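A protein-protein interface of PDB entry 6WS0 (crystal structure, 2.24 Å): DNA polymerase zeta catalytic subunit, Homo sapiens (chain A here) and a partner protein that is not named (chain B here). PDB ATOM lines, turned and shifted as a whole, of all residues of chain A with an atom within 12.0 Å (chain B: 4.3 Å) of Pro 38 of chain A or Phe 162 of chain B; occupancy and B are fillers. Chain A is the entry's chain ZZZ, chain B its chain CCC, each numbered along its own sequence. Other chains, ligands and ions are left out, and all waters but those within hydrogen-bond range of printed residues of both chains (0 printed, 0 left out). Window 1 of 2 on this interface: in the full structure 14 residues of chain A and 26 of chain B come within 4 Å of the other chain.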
ATOM      1  N   LEU A  32       8.031  -0.478   1.749  1.00  0.00           N
ATOM      2  CA  LEU A  32       7.838  -0.992   0.368  1.00  0.00           C
ATOM      3  C   LEU A  32       6.655  -0.252  -0.264  1.00  0.00           C
ATOM      4  O   LEU A  32       5.692   0.039   0.457  1.00  0.00           O
ATOM      5  CB  LEU A  32       7.633  -2.515   0.430  1.00  0.00           C
ATOM      6  CG  LEU A  32       8.885  -3.350   0.733  1.00  0.00           C
ATOM      7  CD1 LEU A  32       8.536  -4.796   1.029  1.00  0.00           C
ATOM      8  CD2 LEU A  32       9.847  -3.307  -0.450  1.00  0.00           C
ATOM      9  N   LYS A  33       6.726   0.041  -1.555  1.00  0.00           N
ATOM     10  CA  LYS A  33       5.604   0.688  -2.266  1.00  0.00           C
ATOM     11  C   LYS A  33       5.582   0.249  -3.720  1.00  0.00           C
ATOM     12  O   LYS A  33       6.625  -0.056  -4.315  1.00  0.00           O
ATOM     13  CB  LYS A  33       5.741   2.206  -2.200  1.00  0.00           C
ATOM     14  CG  LYS A  33       6.887   2.780  -3.011  1.00  0.00           C
ATOM     15  CD  LYS A  33       6.987   4.301  -2.911  1.00  0.00           C
ATOM     16  CE  LYS A  33       5.796   5.012  -3.511  1.00  0.00           C
ATOM     17  NZ  LYS A  33       5.907   4.985  -4.979  1.00  0.00           N
ATOM     18  N   PRO A  34       4.381   0.231  -4.333  1.00  0.00           N
ATOM     19  CA  PRO A  34       4.276  -0.151  -5.729  1.00  0.00           C
ATOM     20  C   PRO A  34       5.079   0.897  -6.491  1.00  0.00           C
ATOM     21  O   PRO A  34       5.006   2.065  -6.176  1.00  0.00           O
ATOM     22  CB  PRO A  34       2.770  -0.127  -6.030  1.00  0.00           C
ATOM     23  CG  PRO A  34       2.100  -0.188  -4.676  1.00  0.00           C
ATOM     24  CD  PRO A  34       3.064   0.513  -3.724  1.00  0.00           C
ATOM     25  N   LEU A  35       5.828   0.460  -7.488  1.00  0.00           N
ATOM     26  CA  LEU A  35       6.464   1.393  -8.450  1.00  0.00           C
ATOM     27  C   LEU A  35       5.361   2.145  -9.204  1.00  0.00           C
ATOM     28  O   LEU A  35       5.563   3.300  -9.626  1.00  0.00           O
ATOM     29  CB  LEU A  35       7.305   0.575  -9.426  1.00  0.00           C
ATOM     30  CG  LEU A  35       8.023   1.397 -10.494  1.00  0.00           C
ATOM     31  CD1 LEU A  35       9.104   2.287  -9.870  1.00  0.00           C
ATOM     32  CD2 LEU A  35       8.625   0.489 -11.544  1.00  0.00           C
ATOM     33  N   MET A  36       4.292   1.444  -9.546  1.00  0.00           N
ATOM     34  CA  MET A  36       3.286   2.007 -10.469  1.00  0.00           C
ATOM     35  C   MET A  36       2.421   2.997  -9.692  1.00  0.00           C
ATOM     36  O   MET A  36       2.210   2.809  -8.472  1.00  0.00           O
ATOM     37  CB  MET A  36       2.438   0.898 -11.089  1.00  0.00           C
ATOM     38  CG  MET A  36       3.273  -0.067 -11.939  1.00  0.00           C
ATOM     39  SD  MET A  36       3.862   0.649 -13.500  1.00  0.00           S
ATOM     40  CE  MET A  36       5.307   1.593 -13.012  1.00  0.00           C
ATOM     41  N   SER A  37       1.972   4.030 -10.379  1.00  0.00           N
ATOM     42  CA  SER A  37       0.941   4.977  -9.878  1.00  0.00           C
ATOM     43  C   SER A  37      -0.439   4.402 -10.168  1.00  0.00           C
ATOM     44  O   SER A  37      -0.608   3.727 -11.174  1.00  0.00           O
ATOM     45  CB  SER A  37       1.142   6.337 -10.507  1.00  0.00           C
ATOM     46  OG  SER A  37       2.237   7.004  -9.883  1.00  0.00           O
ATOM     47  N   PRO A  38      -1.464   4.694  -9.330  1.00  0.00           N
ATOM     48  CA  PRO A  38      -2.852   4.426  -9.710  1.00  0.00           C
ATOM     49  C   PRO A  38      -3.289   5.343 -10.862  1.00  0.00           C
ATOM     50  O   PRO A  38      -2.535   6.170 -11.358  1.00  0.00           O
ATOM     51  CB  PRO A  38      -3.583   4.666  -8.395  1.00  0.00           C
ATOM     52  CG  PRO A  38      -2.802   5.768  -7.780  1.00  0.00           C
ATOM     53  CD  PRO A  38      -1.353   5.437  -8.070  1.00  0.00           C
ATOM     54  N   PRO A  39      -4.448   5.123 -11.490  1.00  0.00           N
ATOM     55  CA  PRO A  39      -4.868   5.991 -12.596  1.00  0.00           C
ATOM     56  C   PRO A  39      -5.107   7.417 -12.096  1.00  0.00           C
ATOM     57  O   PRO A  39      -5.609   7.559 -11.018  1.00  0.00           O
ATOM     58  CB  PRO A  39      -6.160   5.328 -13.093  1.00  0.00           C
ATOM     59  CG  PRO A  39      -6.040   3.899 -12.609  1.00  0.00           C
ATOM     60  CD  PRO A  39      -5.368   4.003 -11.257  1.00  0.00           C
ATOM     61  N   SER A  40      -4.671   8.426 -12.846  1.00  0.00           N
ATOM     62  CA  SER A  40      -4.852   9.853 -12.480  1.00  0.00           C
ATOM     63  C   SER A  40      -6.336  10.182 -12.601  1.00  0.00           C
ATOM     64  O   SER A  40      -7.026   9.546 -13.454  1.00  0.00           O
ATOM     65  CB  SER A  40      -4.011  10.785 -13.326  1.00  0.00           C
ATOM     66  OG  SER A  40      -4.244  10.582 -14.715  1.00  0.00           O
ATOM     67  N   ARG A  41      -6.793  11.109 -11.755  1.00  0.00           N
ATOM     68  CA  ARG A  41      -8.088  11.814 -11.910  1.00  0.00           C
ATOM     69  C   ARG A  41      -8.008  12.596 -13.220  1.00  0.00           C
ATOM     70  O   ARG A  41      -7.452  13.732 -13.206  1.00  0.00           O
ATOM     71  CB  ARG A  41      -8.356  12.744 -10.729  1.00  0.00           C
ATOM     72  CG  ARG A  41      -9.813  13.150 -10.603  1.00  0.00           C
ATOM     73  CD  ARG A  41      -9.970  14.545 -10.058  1.00  0.00           C
ATOM     74  NE  ARG A  41     -11.315  14.744  -9.535  1.00  0.00           N
ATOM     75  CZ  ARG A  41     -11.773  14.237  -8.392  1.00  0.00           C
ATOM     76  NH1 ARG A  41     -10.996  13.481  -7.640  1.00  0.00           N
ATOM     77  NH2 ARG A  41     -13.014  14.471  -8.005  1.00  0.00           N
ATOM     78  N   GLU A  42      -8.508  11.975 -14.291  1.00  0.00           N
ATOM     79  CA  GLU A  42      -8.277  12.354 -15.709  1.00  0.00           C
ATOM     80  C   GLU A  42      -8.491  11.058 -16.490  1.00  0.00           C
ATOM     81  O   GLU A  42      -9.549  10.922 -17.132  1.00  0.00           O
ATOM     82  CB  GLU A  42      -6.875  12.936 -15.968  1.00  0.00           C
ATOM     83  CG  GLU A  42      -6.787  14.462 -15.969  1.00  0.00           C
ATOM     84  CD  GLU A  42      -5.903  15.070 -17.051  1.00  0.00           C
ATOM     85  OE1 GLU A  42      -5.142  14.316 -17.693  1.00  0.00           O
ATOM     86  OE2 GLU A  42      -5.977  16.305 -17.255  1.00  0.00           O
ATOM     87  N   GLU A  43      -7.560  10.111 -16.332  1.00  0.00           N
ATOM     88  CA  GLU A  43      -7.630   8.754 -16.937  1.00  0.00           C
ATOM     89  C   GLU A  43      -9.050   8.204 -16.739  1.00  0.00           C
ATOM     90  O   GLU A  43      -9.620   7.653 -17.709  1.00  0.00           O
ATOM     91  CB  GLU A  43      -6.555   7.837 -16.339  1.00  0.00           C
ATOM     92  CG  GLU A  43      -5.300   7.702 -17.199  1.00  0.00           C
ATOM     93  CD  GLU A  43      -4.041   7.285 -16.450  1.00  0.00           C
ATOM     94  OE1 GLU A  43      -3.373   6.312 -16.870  1.00  0.00           O
ATOM     95  OE2 GLU A  43      -3.722   7.950 -15.450  1.00  0.00           O
ATOM     96  N   ILE A  44      -9.618   8.392 -15.546  1.00  0.00           N
ATOM     97  CA  ILE A  44     -10.904   7.761 -15.131  1.00  0.00           C
ATOM     98  C   ILE A  44     -12.082   8.459 -15.815  1.00  0.00           C
ATOM     99  O   ILE A  44     -12.955   7.730 -16.304  1.00  0.00           O
ATOM    100  CB  ILE A  44     -11.009   7.737 -13.602  1.00  0.00           C
ATOM    101  CG1 ILE A  44     -10.042   6.691 -13.055  1.00  0.00           C
ATOM    102  CG2 ILE A  44     -12.430   7.481 -13.129  1.00  0.00           C
ATOM    103  CD1 ILE A  44      -9.838   6.788 -11.592  1.00  0.00           C
ATOM    104  N   MET A  45     -12.106   9.795 -15.880  1.00  0.00           N
ATOM    105  CA  MET A  45     -13.138  10.533 -16.672  1.00  0.00           C
ATOM    106  C   MET A  45     -12.676  10.640 -18.137  1.00  0.00           C
ATOM    107  O   MET A  45     -12.340  11.756 -18.574  1.00  0.00           O
ATOM    108  CB  MET A  45     -13.452  11.917 -16.079  1.00  0.00           C
ATOM    109  CG  MET A  45     -12.268  12.863 -15.925  1.00  0.00           C
ATOM    110  SD  MET A  45     -12.696  14.355 -14.976  1.00  0.00           S
ATOM    111  CE  MET A  45     -12.452  13.790 -13.294  1.00  0.00           C
ATOM    112  N   LEU B  47     -10.689   6.811  -0.468  1.00  0.00           N
ATOM    113  CA  LEU B  47     -10.628   7.666  -1.688  1.00  0.00           C
ATOM    114  C   LEU B  47     -12.006   8.320  -1.950  1.00  0.00           C
ATOM    115  O   LEU B  47     -12.038   9.454  -2.541  1.00  0.00           O
ATOM    116  CB  LEU B  47     -10.170   6.851  -2.900  1.00  0.00           C
ATOM    117  CG  LEU B  47      -8.902   6.013  -2.735  1.00  0.00           C
ATOM    118  CD1 LEU B  47      -8.859   4.938  -3.817  1.00  0.00           C
ATOM    119  CD2 LEU B  47      -7.635   6.888  -2.805  1.00  0.00           C
ATOM    120  N   TYR B  53     -11.053  10.793  -6.073  1.00  0.00           N
ATOM    121  CA  TYR B  53     -11.706  10.370  -7.333  1.00  0.00           C
ATOM    122  C   TYR B  53     -13.147  10.860  -7.334  1.00  0.00           C
ATOM    123  O   TYR B  53     -13.743  10.935  -6.267  1.00  0.00           O
ATOM    124  CB  TYR B  53     -11.597   8.850  -7.473  1.00  0.00           C
ATOM    125  CG  TYR B  53     -10.211   8.357  -7.805  1.00  0.00           C
ATOM    126  CD1 TYR B  53      -9.676   8.552  -9.068  1.00  0.00           C
ATOM    127  CD2 TYR B  53      -9.415   7.731  -6.857  1.00  0.00           C
ATOM    128  CE1 TYR B  53      -8.398   8.115  -9.386  1.00  0.00           C
ATOM    129  CE2 TYR B  53      -8.141   7.274  -7.160  1.00  0.00           C
ATOM    130  CZ  TYR B  53      -7.630   7.475  -8.428  1.00  0.00           C
ATOM    131  OH  TYR B  53      -6.388   7.026  -8.759  1.00  0.00           O
ATOM    132  N   LEU B  76      -8.542   1.351 -11.508  1.00  0.00           N
ATOM    133  CA  LEU B  76      -8.387   1.705 -10.088  1.00  0.00           C
ATOM    134  C   LEU B  76      -8.639   0.455  -9.265  1.00  0.00           C
ATOM    135  O   LEU B  76      -7.816   0.138  -8.416  1.00  0.00           O
ATOM    136  CB  LEU B  76      -9.373   2.801  -9.722  1.00  0.00           C
ATOM    137  CG  LEU B  76      -9.379   3.165  -8.250  1.00  0.00           C
ATOM    138  CD1 LEU B  76      -8.034   3.783  -7.866  1.00  0.00           C
ATOM    139  CD2 LEU B  76     -10.507   4.140  -7.965  1.00  0.00           C
ATOM    140  N   TYR B  79      -5.547  -1.786  -9.355  1.00  0.00           N
ATOM    141  CA  TYR B  79      -4.385  -1.195  -8.621  1.00  0.00           C
ATOM    142  C   TYR B  79      -4.565  -1.561  -7.145  1.00  0.00           C
ATOM    143  O   TYR B  79      -3.642  -2.091  -6.501  1.00  0.00           O
ATOM    144  CB  TYR B  79      -4.225   0.304  -8.905  1.00  0.00           C
ATOM    145  CG  TYR B  79      -3.081   0.946  -8.150  1.00  0.00           C
ATOM    146  CD1 TYR B  79      -1.881   1.250  -8.778  1.00  0.00           C
ATOM    147  CD2 TYR B  79      -3.169   1.175  -6.790  1.00  0.00           C
ATOM    148  CE1 TYR B  79      -0.815   1.792  -8.075  1.00  0.00           C
ATOM    149  CE2 TYR B  79      -2.100   1.661  -6.067  1.00  0.00           C
ATOM    150  CZ  TYR B  79      -0.928   2.009  -6.716  1.00  0.00           C
ATOM    151  OH  TYR B  79       0.108   2.559  -6.010  1.00  0.00           O
ATOM    152  N   VAL B 102      -1.477   6.850   1.516  1.00  0.00           N
ATOM    153  CA  VAL B 102      -0.897   8.209   1.429  1.00  0.00           C
ATOM    154  C   VAL B 102      -1.623   8.982   0.327  1.00  0.00           C
ATOM    155  O   VAL B 102      -1.596   8.560  -0.868  1.00  0.00           O
ATOM    156  CB  VAL B 102       0.621   8.150   1.140  1.00  0.00           C
ATOM    157  CG1 VAL B 102       1.227   9.539   1.094  1.00  0.00           C
ATOM    158  CG2 VAL B 102       1.381   7.273   2.124  1.00  0.00           C
ATOM    159  N   LEU B 104      -1.244  12.209  -1.844  1.00  0.00           N
ATOM    160  CA  LEU B 104      -0.177  13.023  -2.459  1.00  0.00           C
ATOM    161  C   LEU B 104      -0.839  14.187  -3.195  1.00  0.00           C
ATOM    162  O   LEU B 104      -1.970  13.946  -3.657  1.00  0.00           O
ATOM    163  CB  LEU B 104       0.552  12.140  -3.474  1.00  0.00           C
ATOM    164  CG  LEU B 104       1.202  10.845  -2.999  1.00  0.00           C
ATOM    165  CD1 LEU B 104       1.678  10.081  -4.222  1.00  0.00           C
ATOM    166  CD2 LEU B 104       2.392  11.095  -2.086  1.00  0.00           C
ATOM    167  N   THR B 161      -3.571  12.602  -5.669  1.00  0.00           N
ATOM    168  CA  THR B 161      -3.567  11.167  -6.021  1.00  0.00           C
ATOM    169  C   THR B 161      -3.337  10.411  -4.702  1.00  0.00           C
ATOM    170  O   THR B 161      -3.522  10.997  -3.602  1.00  0.00           O
ATOM    171  CB  THR B 161      -2.539  10.952  -7.149  1.00  0.00           C
ATOM    172  OG1 THR B 161      -1.244  11.324  -6.686  1.00  0.00           O
ATOM    173  CG2 THR B 161      -2.762  11.836  -8.358  1.00  0.00           C
ATOM    174  N   PHE B 162      -2.947   9.145  -4.782  1.00  0.00           N
ATOM    175  CA  PHE B 162      -2.533   8.380  -3.590  1.00  0.00           C
ATOM    176  C   PHE B 162      -1.494   7.343  -3.977  1.00  0.00           C
ATOM    177  O   PHE B 162      -1.257   7.065  -5.165  1.00  0.00           O
ATOM    178  CB  PHE B 162      -3.739   7.707  -2.944  1.00  0.00           C
ATOM    179  CG  PHE B 162      -4.223   6.471  -3.659  1.00  0.00           C
ATOM    180  CD1 PHE B 162      -4.914   6.567  -4.854  1.00  0.00           C
ATOM    181  CD2 PHE B 162      -4.004   5.222  -3.116  1.00  0.00           C
ATOM    182  CE1 PHE B 162      -5.413   5.442  -5.486  1.00  0.00           C
ATOM    183  CE2 PHE B 162      -4.430   4.098  -3.795  1.00  0.00           C
ATOM    184  CZ  PHE B 162      -5.157   4.209  -4.954  1.00  0.00           C
ATOM    185  N   THR B 163      -1.004   6.691  -2.948  1.00  0.00           N
ATOM    186  CA  THR B 163      -0.185   5.487  -3.072  1.00  0.00           C
ATOM    187  C   THR B 163      -0.338   4.682  -1.799  1.00  0.00           C
ATOM    188  O   THR B 163      -1.112   5.101  -0.932  1.00  0.00           O
ATOM    189  CB  THR B 163       1.277   5.856  -3.294  1.00  0.00           C
ATOM    190  OG1 THR B 163       1.907   4.643  -3.712  1.00  0.00           O
ATOM    191  CG2 THR B 163       1.876   6.451  -2.034  1.00  0.00           C
ATOM    192  N   VAL B 164       0.371   3.558  -1.719  1.00  0.00           N
ATOM    193  CA  VAL B 164       0.265   2.623  -0.571  1.00  0.00           C
ATOM    194  C   VAL B 164       1.701   2.335  -0.152  1.00  0.00           C
ATOM    195  O   VAL B 164       2.557   2.172  -1.043  1.00  0.00           O
ATOM    196  CB  VAL B 164      -0.549   1.352  -0.867  1.00  0.00           C
ATOM    197  CG1 VAL B 164      -0.589   0.411   0.329  1.00  0.00           C
ATOM    198  CG2 VAL B 164      -1.976   1.668  -1.269  1.00  0.00           C
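Of the 10 printed residues of chain B, 6 touch a printed residue of chain A. Hydrophobic or aromatic side chains of chain B that line the printed part of chain A: Tyr 53, Tyr 79 and Phe 162. Hydrophobic or aromatic side chains of chain A within 4 Å of the printed part of chain B: Pro 34, Pro 38, Pro 39 and Ile 44. Among the printed residues, 13 pairs touch across the chains.
The backbone carbonyl oxygen (O) of Val 102 of chain B lies within hydrogen-bond range of the backbone NH (N) of Thr 163 of chain B (2.9 Å).
Among the printed residues, pairs that only touch across the chains: Lys 33 of chain A with Thr 163 of chain B (3.9 Å), Lys 33 of chain A with Val 164 of chain B (3.4 Å), Pro 34 of chain A with Tyr 79 of chain B (3.6 Å), Pro 34 of chain A with Val 164 of chain B (3.2 Å), Ser 37 of chain A with Tyr 79 of chain B (3.4 Å), Pro 38 of chain A with Tyr 53 of chain B (3.7 Å), Pro 38 of chain A with Tyr 79 of chain B (3.2 Å), Pro 38 of chain A with Phe 162 of chain B (3.3 Å), Pro 39 of chain A with Leu 76 of chain B (3.7 Å) and Ile 44 of chain A with Tyr 53 of chain B (2.9 Å).
Printed residues of chain B within 4 Å of Pro 34 of chain A: Tyr 79 and Val 164. Leu 35 of chain A touches none of the printed residues of chain B. Printed residues of chain B within 4 Å of Met 36 of chain A: Tyr 79. Pro 38 of chain A touches just these residues of chain B: Tyr 53, Tyr 79 and Phe 162. Printed residues of chain B within 4 Å of Pro 39 of chain A: Tyr 53 (2.4 Å) and Leu 76 (3.7 Å). Printed residues of chain B within 4 Å of Ile 44 of chain A: Tyr 53. Of the printed residues of chain A, Tyr 53 of chain B touches Pro 38 (3.7 Å), Pro 39 (2.4 Å), Arg 41 (3.1 Å) and Ile 44 (2.9 Å). Of the printed residues of chain A, Leu 76 of chain B touches Pro 39 (3.7 Å). No residue of chain A comes within 4 Å of Val 102 of chain B. No residue of chain A comes within 4 Å of Thr 161 of chain B. Phe 162 of chain B touches just one residue of chain A: Pro 38. The nearest printed residue of chain B that does not touch Pro 38 of chain A is Leu 76 of chain B (4.6 Å). The nearest printed residue of chain B that does not touch Arg 41 of chain A is Thr 161 of chain B (5.3 Å).
The side-chain hydroxyl of Tyr 53 of chain B is in hydrogen-bond range of the backbone carbonyl oxygen of Pro 39 of chain A, 2.4 Å away. OH of Tyr 79 of chain B sits close to O of Met 36 of chain A, at 3.2 Å. The backbone NH (N) of Tyr 53 of chain B sits close to the guanidinium group (NH1) of Arg 41 of chain A (3.1 Å).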
